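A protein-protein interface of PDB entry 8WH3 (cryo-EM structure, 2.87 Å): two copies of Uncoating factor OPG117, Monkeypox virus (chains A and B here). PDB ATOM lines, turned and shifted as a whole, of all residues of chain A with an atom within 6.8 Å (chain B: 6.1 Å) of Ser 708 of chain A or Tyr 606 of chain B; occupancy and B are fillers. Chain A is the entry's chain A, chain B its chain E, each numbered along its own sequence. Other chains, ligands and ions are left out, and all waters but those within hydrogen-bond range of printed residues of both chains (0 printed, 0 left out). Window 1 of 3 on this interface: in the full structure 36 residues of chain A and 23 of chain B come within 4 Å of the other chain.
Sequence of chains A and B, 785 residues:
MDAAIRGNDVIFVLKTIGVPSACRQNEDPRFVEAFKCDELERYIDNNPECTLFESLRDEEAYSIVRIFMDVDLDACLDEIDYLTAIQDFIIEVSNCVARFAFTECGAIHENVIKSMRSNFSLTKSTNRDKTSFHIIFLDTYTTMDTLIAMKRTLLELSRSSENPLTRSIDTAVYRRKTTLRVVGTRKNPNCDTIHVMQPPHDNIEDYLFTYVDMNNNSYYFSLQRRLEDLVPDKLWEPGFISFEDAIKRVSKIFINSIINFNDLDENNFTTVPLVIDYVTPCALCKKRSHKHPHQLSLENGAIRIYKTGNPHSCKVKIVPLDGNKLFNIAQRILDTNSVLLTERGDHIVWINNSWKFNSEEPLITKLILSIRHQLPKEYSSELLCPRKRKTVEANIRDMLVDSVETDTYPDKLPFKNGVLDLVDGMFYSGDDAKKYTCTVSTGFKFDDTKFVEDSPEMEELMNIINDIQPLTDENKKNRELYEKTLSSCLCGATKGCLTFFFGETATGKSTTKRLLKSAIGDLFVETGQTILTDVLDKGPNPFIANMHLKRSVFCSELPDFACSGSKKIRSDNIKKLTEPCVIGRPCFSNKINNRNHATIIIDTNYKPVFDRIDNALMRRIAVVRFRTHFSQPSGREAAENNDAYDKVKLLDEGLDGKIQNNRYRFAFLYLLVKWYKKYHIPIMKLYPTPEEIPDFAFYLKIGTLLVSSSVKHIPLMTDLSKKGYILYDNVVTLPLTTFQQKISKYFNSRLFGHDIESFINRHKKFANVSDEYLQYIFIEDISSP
The backbone carbonyl oxygen (O) of Ser 708 of chain A lies within hydrogen-bond range of the side-chain amide nitrogen (ND2) of Asn 642 of chain B, at 3.5 Å. O of Ala 638 of chain B is in hydrogen-bond range of OG of Ser 710 of chain A. The backbone NH of Asn 641 of chain B sits at hydrogen-bond distance from the side-chain hydroxyl of Ser 710 of chain A (2.9 Å). OG of Ser 710 of chain A sits at hydrogen-bond distance from N of Asn 642 of chain B, 2.4 Å away. The side-chain amide nitrogen (NE2) of Gln 775 of chain A is in hydrogen-bond range of the side-chain amide oxygen (OD1) of Asn 642 of chain B, at 3.1 Å.
Among the printed residues, pairs that only touch across the chains: Val 707 of chain A with Ala 638 of chain B (3.8 Å), Ser 708 of chain A with Tyr 606 of chain B (3.7 Å), Ser 709 of chain A with Tyr 606 of chain B (3.9 Å), Ser 709 of chain A with Asn 642 of chain B (3.5 Å), Ile 777 of chain A with Asn 641 of chain B (3.3 Å), Ile 777 of chain A with Asn 642 of chain B (3.3 Å) and Ile 782 of chain A with Asn 641 of chain B (3.1 Å).
The backbone NH of Val 707 of chain A sits at hydrogen-bond distance from the backbone carbonyl oxygen of Ile 777 of chain A (3.2 Å). O of Tyr 606 of chain B sits at hydrogen-bond distance from OG1 of Thr 604 of chain B, 2.6 Å away.
Of the 9 printed residues of chain A, 7 touch a printed residue of chain B. Of the 16 printed residues of chain B, 4 touch a printed residue of chain A. Along chain B the printed residues that touch a printed residue of chain A span positions 606 to 642.
Ser 708 of chain A touches just these residues of chain B: Tyr 606 and Asn 642. Of chain A, only Ser 708 (3.7 Å) and Ser 709 (3.9 Å) come within 4 Å of Tyr 606 of chain B. Printed residues of chain B within 4 Å of Gln 775 of chain A: Asn 642 (3.1 Å). Printed residues of chain B within 4 Å of Ile 777 of chain A: Asn 641 and Asn 642. Printed residues of chain A within 4 Å of Asn 641 of chain B: Ser 710 (2.9 Å), Ile 777 (3.3 Å) and Ile 782 (3.1 Å). Tyr 776 of chain A touches none of the printed residues of chain B. Phe 502 of chain B touches none of the printed residues of chain A. The nearest residue of chain B that does not touch Ser 708 of chain A is Ala 638 of chain B (4.7 Å).
No position is printed for both chains.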
ATOM      1  N   LEU A 706      12.165   8.957  -6.198  1.00  0.00           N
ATOM      2  CA  LEU A 706      10.817   9.436  -5.935  1.00  0.00           C
ATOM      3  C   LEU A 706       9.813   8.323  -6.195  1.00  0.00           C
ATOM      4  O   LEU A 706      10.069   7.402  -6.976  1.00  0.00           O
ATOM      5  CB  LEU A 706      10.473  10.651  -6.805  1.00  0.00           C
ATOM      6  CG  LEU A 706      11.535  11.745  -6.924  1.00  0.00           C
ATOM      7  CD1 LEU A 706      11.044  12.862  -7.828  1.00  0.00           C
ATOM      8  CD2 LEU A 706      11.905  12.283  -5.553  1.00  0.00           C
ATOM      9  N   VAL A 707       8.665   8.416  -5.527  1.00  0.00           N
ATOM     10  CA  VAL A 707       7.570   7.476  -5.712  1.00  0.00           C
ATOM     11  C   VAL A 707       6.293   8.269  -5.948  1.00  0.00           C
ATOM     12  O   VAL A 707       6.191   9.449  -5.606  1.00  0.00           O
ATOM     13  CB  VAL A 707       7.394   6.526  -4.509  1.00  0.00           C
ATOM     14  CG1 VAL A 707       8.570   5.567  -4.408  1.00  0.00           C
ATOM     15  CG2 VAL A 707       7.230   7.323  -3.227  1.00  0.00           C
ATOM     16  N   SER A 708       5.311   7.600  -6.540  1.00  0.00           N
ATOM     17  CA  SER A 708       4.021   8.215  -6.805  1.00  0.00           C
ATOM     18  C   SER A 708       3.150   8.110  -5.555  1.00  0.00           C
ATOM     19  O   SER A 708       3.614   7.739  -4.473  1.00  0.00           O
ATOM     20  CB  SER A 708       3.366   7.566  -8.022  1.00  0.00           C
ATOM     21  OG  SER A 708       4.019   7.949  -9.221  1.00  0.00           O
ATOM     22  N   SER A 709       1.872   8.450  -5.692  1.00  0.00           N
ATOM     23  CA  SER A 709       0.947   8.370  -4.571  1.00  0.00           C
ATOM     24  C   SER A 709       0.679   6.916  -4.193  1.00  0.00           C
ATOM     25  O   SER A 709       0.781   6.005  -5.019  1.00  0.00           O
ATOM     26  CB  SER A 709      -0.354   9.086  -4.919  1.00  0.00           C
ATOM     27  OG  SER A 709      -0.741   8.815  -6.255  1.00  0.00           O
ATOM     28  N   SER A 710       0.330   6.702  -2.929  1.00  0.00           N
ATOM     29  CA  SER A 710       0.251   5.358  -2.366  1.00  0.00           C
ATOM     30  C   SER A 710      -0.836   5.340  -1.292  1.00  0.00           C
ATOM     31  O   SER A 710      -1.711   6.209  -1.269  1.00  0.00           O
ATOM     32  CB  SER A 710       1.630   4.900  -1.858  1.00  0.00           C
ATOM     33  OG  SER A 710       2.130   5.709  -0.816  1.00  0.00           O
ATOM     34  N   GLN A 775       3.626  16.445  -6.297  1.00  0.00           N
ATOM     35  CA  GLN A 775       3.144  15.226  -5.653  1.00  0.00           C
ATOM     36  C   GLN A 775       4.187  14.126  -5.847  1.00  0.00           C
ATOM     37  O   GLN A 775       4.027  13.205  -6.647  1.00  0.00           O
ATOM     38  CB  GLN A 775       1.787  14.828  -6.233  1.00  0.00           C
ATOM     39  CG  GLN A 775       0.775  14.102  -5.308  1.00  0.00           C
ATOM     40  CD  GLN A 775       1.258  12.839  -4.595  1.00  0.00           C
ATOM     41  OE1 GLN A 775       2.306  12.287  -4.891  1.00  0.00           O
ATOM     42  NE2 GLN A 775       0.439  12.357  -3.671  1.00  0.00           N
ATOM     43  N   TYR A 776       5.310  14.288  -5.149  1.00  0.00           N
ATOM     44  CA  TYR A 776       6.384  13.305  -5.141  1.00  0.00           C
ATOM     45  C   TYR A 776       6.988  13.253  -3.746  1.00  0.00           C
ATOM     46  O   TYR A 776       7.078  14.273  -3.058  1.00  0.00           O
ATOM     47  CB  TYR A 776       7.479  13.631  -6.173  1.00  0.00           C
ATOM     48  CG  TYR A 776       7.131  13.227  -7.589  1.00  0.00           C
ATOM     49  CD1 TYR A 776       6.552  11.993  -7.855  1.00  0.00           C
ATOM     50  CD2 TYR A 776       7.379  14.077  -8.659  1.00  0.00           C
ATOM     51  CE1 TYR A 776       6.227  11.617  -9.144  1.00  0.00           C
ATOM     52  CE2 TYR A 776       7.058  13.710  -9.954  1.00  0.00           C
ATOM     53  CZ  TYR A 776       6.482  12.478 -10.190  1.00  0.00           C
ATOM     54  OH  TYR A 776       6.159  12.107 -11.475  1.00  0.00           O
ATOM     55  N   ILE A 777       7.407  12.057  -3.336  1.00  0.00           N
ATOM     56  CA  ILE A 777       8.000  11.836  -2.022  1.00  0.00           C
ATOM     57  C   ILE A 777       9.350  11.158  -2.205  1.00  0.00           C
ATOM     58  O   ILE A 777       9.450  10.145  -2.906  1.00  0.00           O
ATOM     59  CB  ILE A 777       7.090  10.985  -1.114  1.00  0.00           C
ATOM     60  CG1 ILE A 777       5.653  11.515  -1.145  1.00  0.00           C
ATOM     61  CG2 ILE A 777       7.640  10.953   0.308  1.00  0.00           C
ATOM     62  CD1 ILE A 777       4.818  11.124   0.059  1.00  0.00           C
ATOM     63  N   ILE A 782      11.379   8.397   3.086  1.00  0.00           N
ATOM     64  CA  ILE A 782      10.534   7.241   3.363  1.00  0.00           C
ATOM     65  C   ILE A 782      11.312   6.162   4.106  1.00  0.00           C
ATOM     66  O   ILE A 782      10.823   5.595   5.091  1.00  0.00           O
ATOM     67  CB  ILE A 782       9.938   6.711   2.046  1.00  0.00           C
ATOM     68  CG1 ILE A 782       9.021   7.762   1.415  1.00  0.00           C
ATOM     69  CG2 ILE A 782       9.226   5.393   2.263  1.00  0.00           C
ATOM     70  CD1 ILE A 782       8.214   7.246   0.252  1.00  0.00           C
ATOM     71  N   PHE B 502     -11.831   4.422 -11.942  1.00  0.00           N
ATOM     72  CA  PHE B 502     -10.951   5.147 -11.031  1.00  0.00           C
ATOM     73  C   PHE B 502     -10.253   4.128 -10.145  1.00  0.00           C
ATOM     74  O   PHE B 502     -10.764   3.736  -9.094  1.00  0.00           O
ATOM     75  CB  PHE B 502     -11.742   6.155 -10.208  1.00  0.00           C
ATOM     76  CG  PHE B 502     -10.900   7.243  -9.601  1.00  0.00           C
ATOM     77  CD1 PHE B 502      -9.532   7.284  -9.810  1.00  0.00           C
ATOM     78  CD2 PHE B 502     -11.481   8.230  -8.824  1.00  0.00           C
ATOM     79  CE1 PHE B 502      -8.761   8.283  -9.253  1.00  0.00           C
ATOM     80  CE2 PHE B 502     -10.716   9.233  -8.264  1.00  0.00           C
ATOM     81  CZ  PHE B 502      -9.354   9.259  -8.478  1.00  0.00           C
ATOM     82  N   GLY B 503      -9.072   3.703 -10.575  1.00  0.00           N
ATOM     83  CA  GLY B 503      -8.303   2.711  -9.859  1.00  0.00           C
ATOM     84  C   GLY B 503      -6.822   2.960 -10.033  1.00  0.00           C
ATOM     85  O   GLY B 503      -6.384   3.438 -11.082  1.00  0.00           O
ATOM     86  N   GLU B 504      -6.039   2.644  -9.010  1.00  0.00           N
ATOM     87  CA  GLU B 504      -4.632   2.992  -9.031  1.00  0.00           C
ATOM     88  C   GLU B 504      -3.801   1.836  -9.591  1.00  0.00           C
ATOM     89  O   GLU B 504      -4.307   0.750  -9.885  1.00  0.00           O
ATOM     90  CB  GLU B 504      -4.153   3.370  -7.632  1.00  0.00           C
ATOM     91  CG  GLU B 504      -5.130   4.204  -6.788  1.00  0.00           C
ATOM     92  CD  GLU B 504      -6.288   3.394  -6.213  1.00  0.00           C
ATOM     93  OE1 GLU B 504      -6.472   3.410  -4.980  1.00  0.00           O
ATOM     94  OE2 GLU B 504      -7.019   2.745  -6.987  1.00  0.00           O
ATOM     95  N   THR B 505      -2.503   2.087  -9.730  1.00  0.00           N
ATOM     96  CA  THR B 505      -1.594   1.104 -10.303  1.00  0.00           C
ATOM     97  C   THR B 505      -1.476  -0.121  -9.400  1.00  0.00           C
ATOM     98  O   THR B 505      -1.396  -0.012  -8.173  1.00  0.00           O
ATOM     99  CB  THR B 505      -0.216   1.735 -10.531  1.00  0.00           C
ATOM    100  OG1 THR B 505      -0.226   2.475 -11.758  1.00  0.00           O
ATOM    101  CG2 THR B 505       0.878   0.675 -10.597  1.00  0.00           C
ATOM    102  N   LEU B 558      -2.906   5.928 -19.024  1.00  0.00           N
ATOM    103  CA  LEU B 558      -3.213   7.347 -19.149  1.00  0.00           C
ATOM    104  C   LEU B 558      -2.364   8.158 -18.179  1.00  0.00           C
ATOM    105  O   LEU B 558      -2.384   7.883 -16.972  1.00  0.00           O
ATOM    106  CB  LEU B 558      -4.695   7.586 -18.892  1.00  0.00           C
ATOM    107  CG  LEU B 558      -5.621   7.132 -20.022  1.00  0.00           C
ATOM    108  CD1 LEU B 558      -7.045   7.584 -19.767  1.00  0.00           C
ATOM    109  CD2 LEU B 558      -5.122   7.649 -21.361  1.00  0.00           C
ATOM    110  N   PRO B 559      -1.608   9.146 -18.650  1.00  0.00           N
ATOM    111  CA  PRO B 559      -0.801   9.967 -17.743  1.00  0.00           C
ATOM    112  C   PRO B 559      -1.661  10.898 -16.903  1.00  0.00           C
ATOM    113  O   PRO B 559      -2.826  11.164 -17.204  1.00  0.00           O
ATOM    114  CB  PRO B 559       0.104  10.766 -18.691  1.00  0.00           C
ATOM    115  CG  PRO B 559      -0.017  10.086 -20.029  1.00  0.00           C
ATOM    116  CD  PRO B 559      -1.391   9.512 -20.056  1.00  0.00           C
ATOM    117  N   ASP B 560      -1.056  11.395 -15.828  1.00  0.00           N
ATOM    118  CA  ASP B 560      -1.753  12.305 -14.928  1.00  0.00           C
ATOM    119  C   ASP B 560      -2.017  13.634 -15.623  1.00  0.00           C
ATOM    120  O   ASP B 560      -1.092  14.282 -16.124  1.00  0.00           O
ATOM    121  CB  ASP B 560      -0.932  12.527 -13.658  1.00  0.00           C
ATOM    122  N   PHE B 561      -3.283  14.040 -15.655  1.00  0.00           N
ATOM    123  CA  PHE B 561      -3.676  15.293 -16.282  1.00  0.00           C
ATOM    124  C   PHE B 561      -3.574  16.487 -15.343  1.00  0.00           C
ATOM    125  O   PHE B 561      -3.682  17.629 -15.806  1.00  0.00           O
ATOM    126  CB  PHE B 561      -5.108  15.186 -16.816  1.00  0.00           C
ATOM    127  CG  PHE B 561      -5.301  14.078 -17.811  1.00  0.00           C
ATOM    128  CD1 PHE B 561      -4.721  14.147 -19.065  1.00  0.00           C
ATOM    129  CD2 PHE B 561      -6.058  12.964 -17.489  1.00  0.00           C
ATOM    130  CE1 PHE B 561      -4.898  13.128 -19.982  1.00  0.00           C
ATOM    131  CE2 PHE B 561      -6.236  11.942 -18.401  1.00  0.00           C
ATOM    132  CZ  PHE B 561      -5.654  12.024 -19.649  1.00  0.00           C
ATOM    133  N   THR B 604      -7.459   5.439 -15.269  1.00  0.00           N
ATOM    134  CA  THR B 604      -6.468   6.397 -14.800  1.00  0.00           C
ATOM    135  C   THR B 604      -6.099   6.093 -13.357  1.00  0.00           C
ATOM    136  O   THR B 604      -6.940   5.671 -12.560  1.00  0.00           O
ATOM    137  CB  THR B 604      -6.971   7.847 -14.885  1.00  0.00           C
ATOM    138  OG1 THR B 604      -7.918   8.088 -13.838  1.00  0.00           O
ATOM    139  CG2 THR B 604      -7.615   8.124 -16.227  1.00  0.00           C
ATOM    140  N   ASN B 605      -4.832   6.326 -13.027  1.00  0.00           N
ATOM    141  CA  ASN B 605      -4.342   6.188 -11.663  1.00  0.00           C
ATOM    142  C   ASN B 605      -4.552   7.445 -10.833  1.00  0.00           C
ATOM    143  O   ASN B 605      -4.227   7.448  -9.643  1.00  0.00           O
ATOM    144  CB  ASN B 605      -2.853   5.827 -11.669  1.00  0.00           C
ATOM    145  CG  ASN B 605      -2.569   4.525 -12.387  1.00  0.00           C
ATOM    146  OD1 ASN B 605      -3.259   3.526 -12.180  1.00  0.00           O
ATOM    147  ND2 ASN B 605      -1.547   4.528 -13.234  1.00  0.00           N
ATOM    148  N   TYR B 606      -5.084   8.508 -11.433  1.00  0.00           N
ATOM    149  CA  TYR B 606      -5.240   9.790 -10.763  1.00  0.00           C
ATOM    150  C   TYR B 606      -6.595  10.376 -11.130  1.00  0.00           C
ATOM    151  O   TYR B 606      -7.219   9.976 -12.115  1.00  0.00           O
ATOM    152  CB  TYR B 606      -4.114  10.760 -11.147  1.00  0.00           C
ATOM    153  CG  TYR B 606      -2.745  10.119 -11.177  1.00  0.00           C
ATOM    154  CD1 TYR B 606      -2.242   9.564 -12.347  1.00  0.00           C
ATOM    155  CD2 TYR B 606      -1.958  10.060 -10.034  1.00  0.00           C
ATOM    156  CE1 TYR B 606      -0.993   8.975 -12.380  1.00  0.00           C
ATOM    157  CE2 TYR B 606      -0.707   9.471 -10.058  1.00  0.00           C
ATOM    158  CZ  TYR B 606      -0.230   8.931 -11.233  1.00  0.00           C
ATOM    159  OH  TYR B 606       1.014   8.344 -11.261  1.00  0.00           O
ATOM    160  N   LYS B 607      -7.048  11.329 -10.318  1.00  0.00           N
ATOM    161  CA  LYS B 607      -8.346  11.938 -10.552  1.00  0.00           C
ATOM    162  C   LYS B 607      -8.335  12.709 -11.873  1.00  0.00           C
ATOM    163  O   LYS B 607      -7.310  13.274 -12.265  1.00  0.00           O
ATOM    164  CB  LYS B 607      -8.724  12.860  -9.392  1.00  0.00           C
ATOM    165  CG  LYS B 607      -8.004  14.196  -9.363  1.00  0.00           C
ATOM    166  CD  LYS B 607      -8.553  15.085  -8.259  1.00  0.00           C
ATOM    167  CE  LYS B 607      -8.626  16.538  -8.697  1.00  0.00           C
ATOM    168  NZ  LYS B 607      -9.586  16.732  -9.817  1.00  0.00           N
ATOM    169  N   PRO B 608      -9.454  12.729 -12.591  1.00  0.00           N
ATOM    170  CA  PRO B 608      -9.477  13.363 -13.910  1.00  0.00           C
ATOM    171  C   PRO B 608      -9.583  14.878 -13.816  1.00  0.00           C
ATOM    172  O   PRO B 608     -10.103  15.441 -12.852  1.00  0.00           O
ATOM    173  CB  PRO B 608     -10.722  12.767 -14.579  1.00  0.00           C
ATOM    174  CG  PRO B 608     -11.527  12.134 -13.475  1.00  0.00           C
ATOM    175  CD  PRO B 608     -10.781  12.240 -12.183  1.00  0.00           C
ATOM    176  N   ALA B 638       6.851   2.229   0.555  1.00  0.00           N
ATOM    177  CA  ALA B 638       6.591   3.330  -0.365  1.00  0.00           C
ATOM    178  C   ALA B 638       5.218   3.206  -1.010  1.00  0.00           C
ATOM    179  O   ALA B 638       4.666   4.206  -1.482  1.00  0.00           O
ATOM    180  CB  ALA B 638       7.680   3.389  -1.436  1.00  0.00           C
ATOM    181  N   ASN B 641       3.078   4.907   1.843  1.00  0.00           N
ATOM    182  CA  ASN B 641       3.396   6.209   2.423  1.00  0.00           C
ATOM    183  C   ASN B 641       2.933   7.397   1.583  1.00  0.00           C
ATOM    184  O   ASN B 641       3.641   8.404   1.495  1.00  0.00           O
ATOM    185  CB  ASN B 641       4.900   6.334   2.675  1.00  0.00           C
ATOM    186  CG  ASN B 641       5.390   5.369   3.730  1.00  0.00           C
ATOM    187  OD1 ASN B 641       6.556   4.983   3.739  1.00  0.00           O
ATOM    188  ND2 ASN B 641       4.478   4.904   4.574  1.00  0.00           N
ATOM    189  N   ASN B 642       1.755   7.307   0.977  1.00  0.00           N
ATOM    190  CA  ASN B 642       1.145   8.459   0.307  1.00  0.00           C
ATOM    191  C   ASN B 642      -0.371   8.272   0.356  1.00  0.00           C
ATOM    192  O   ASN B 642      -0.889   7.552   1.214  1.00  0.00           O
ATOM    193  CB  ASN B 642       1.716   8.644  -1.108  1.00  0.00           C
ATOM    194  CG  ASN B 642       1.840  10.100  -1.504  1.00  0.00           C
ATOM    195  OD1 ASN B 642       1.115  10.956  -1.000  1.00  0.00           O
ATOM    196  ND2 ASN B 642       2.755  10.387  -2.423  1.00  0.00           N
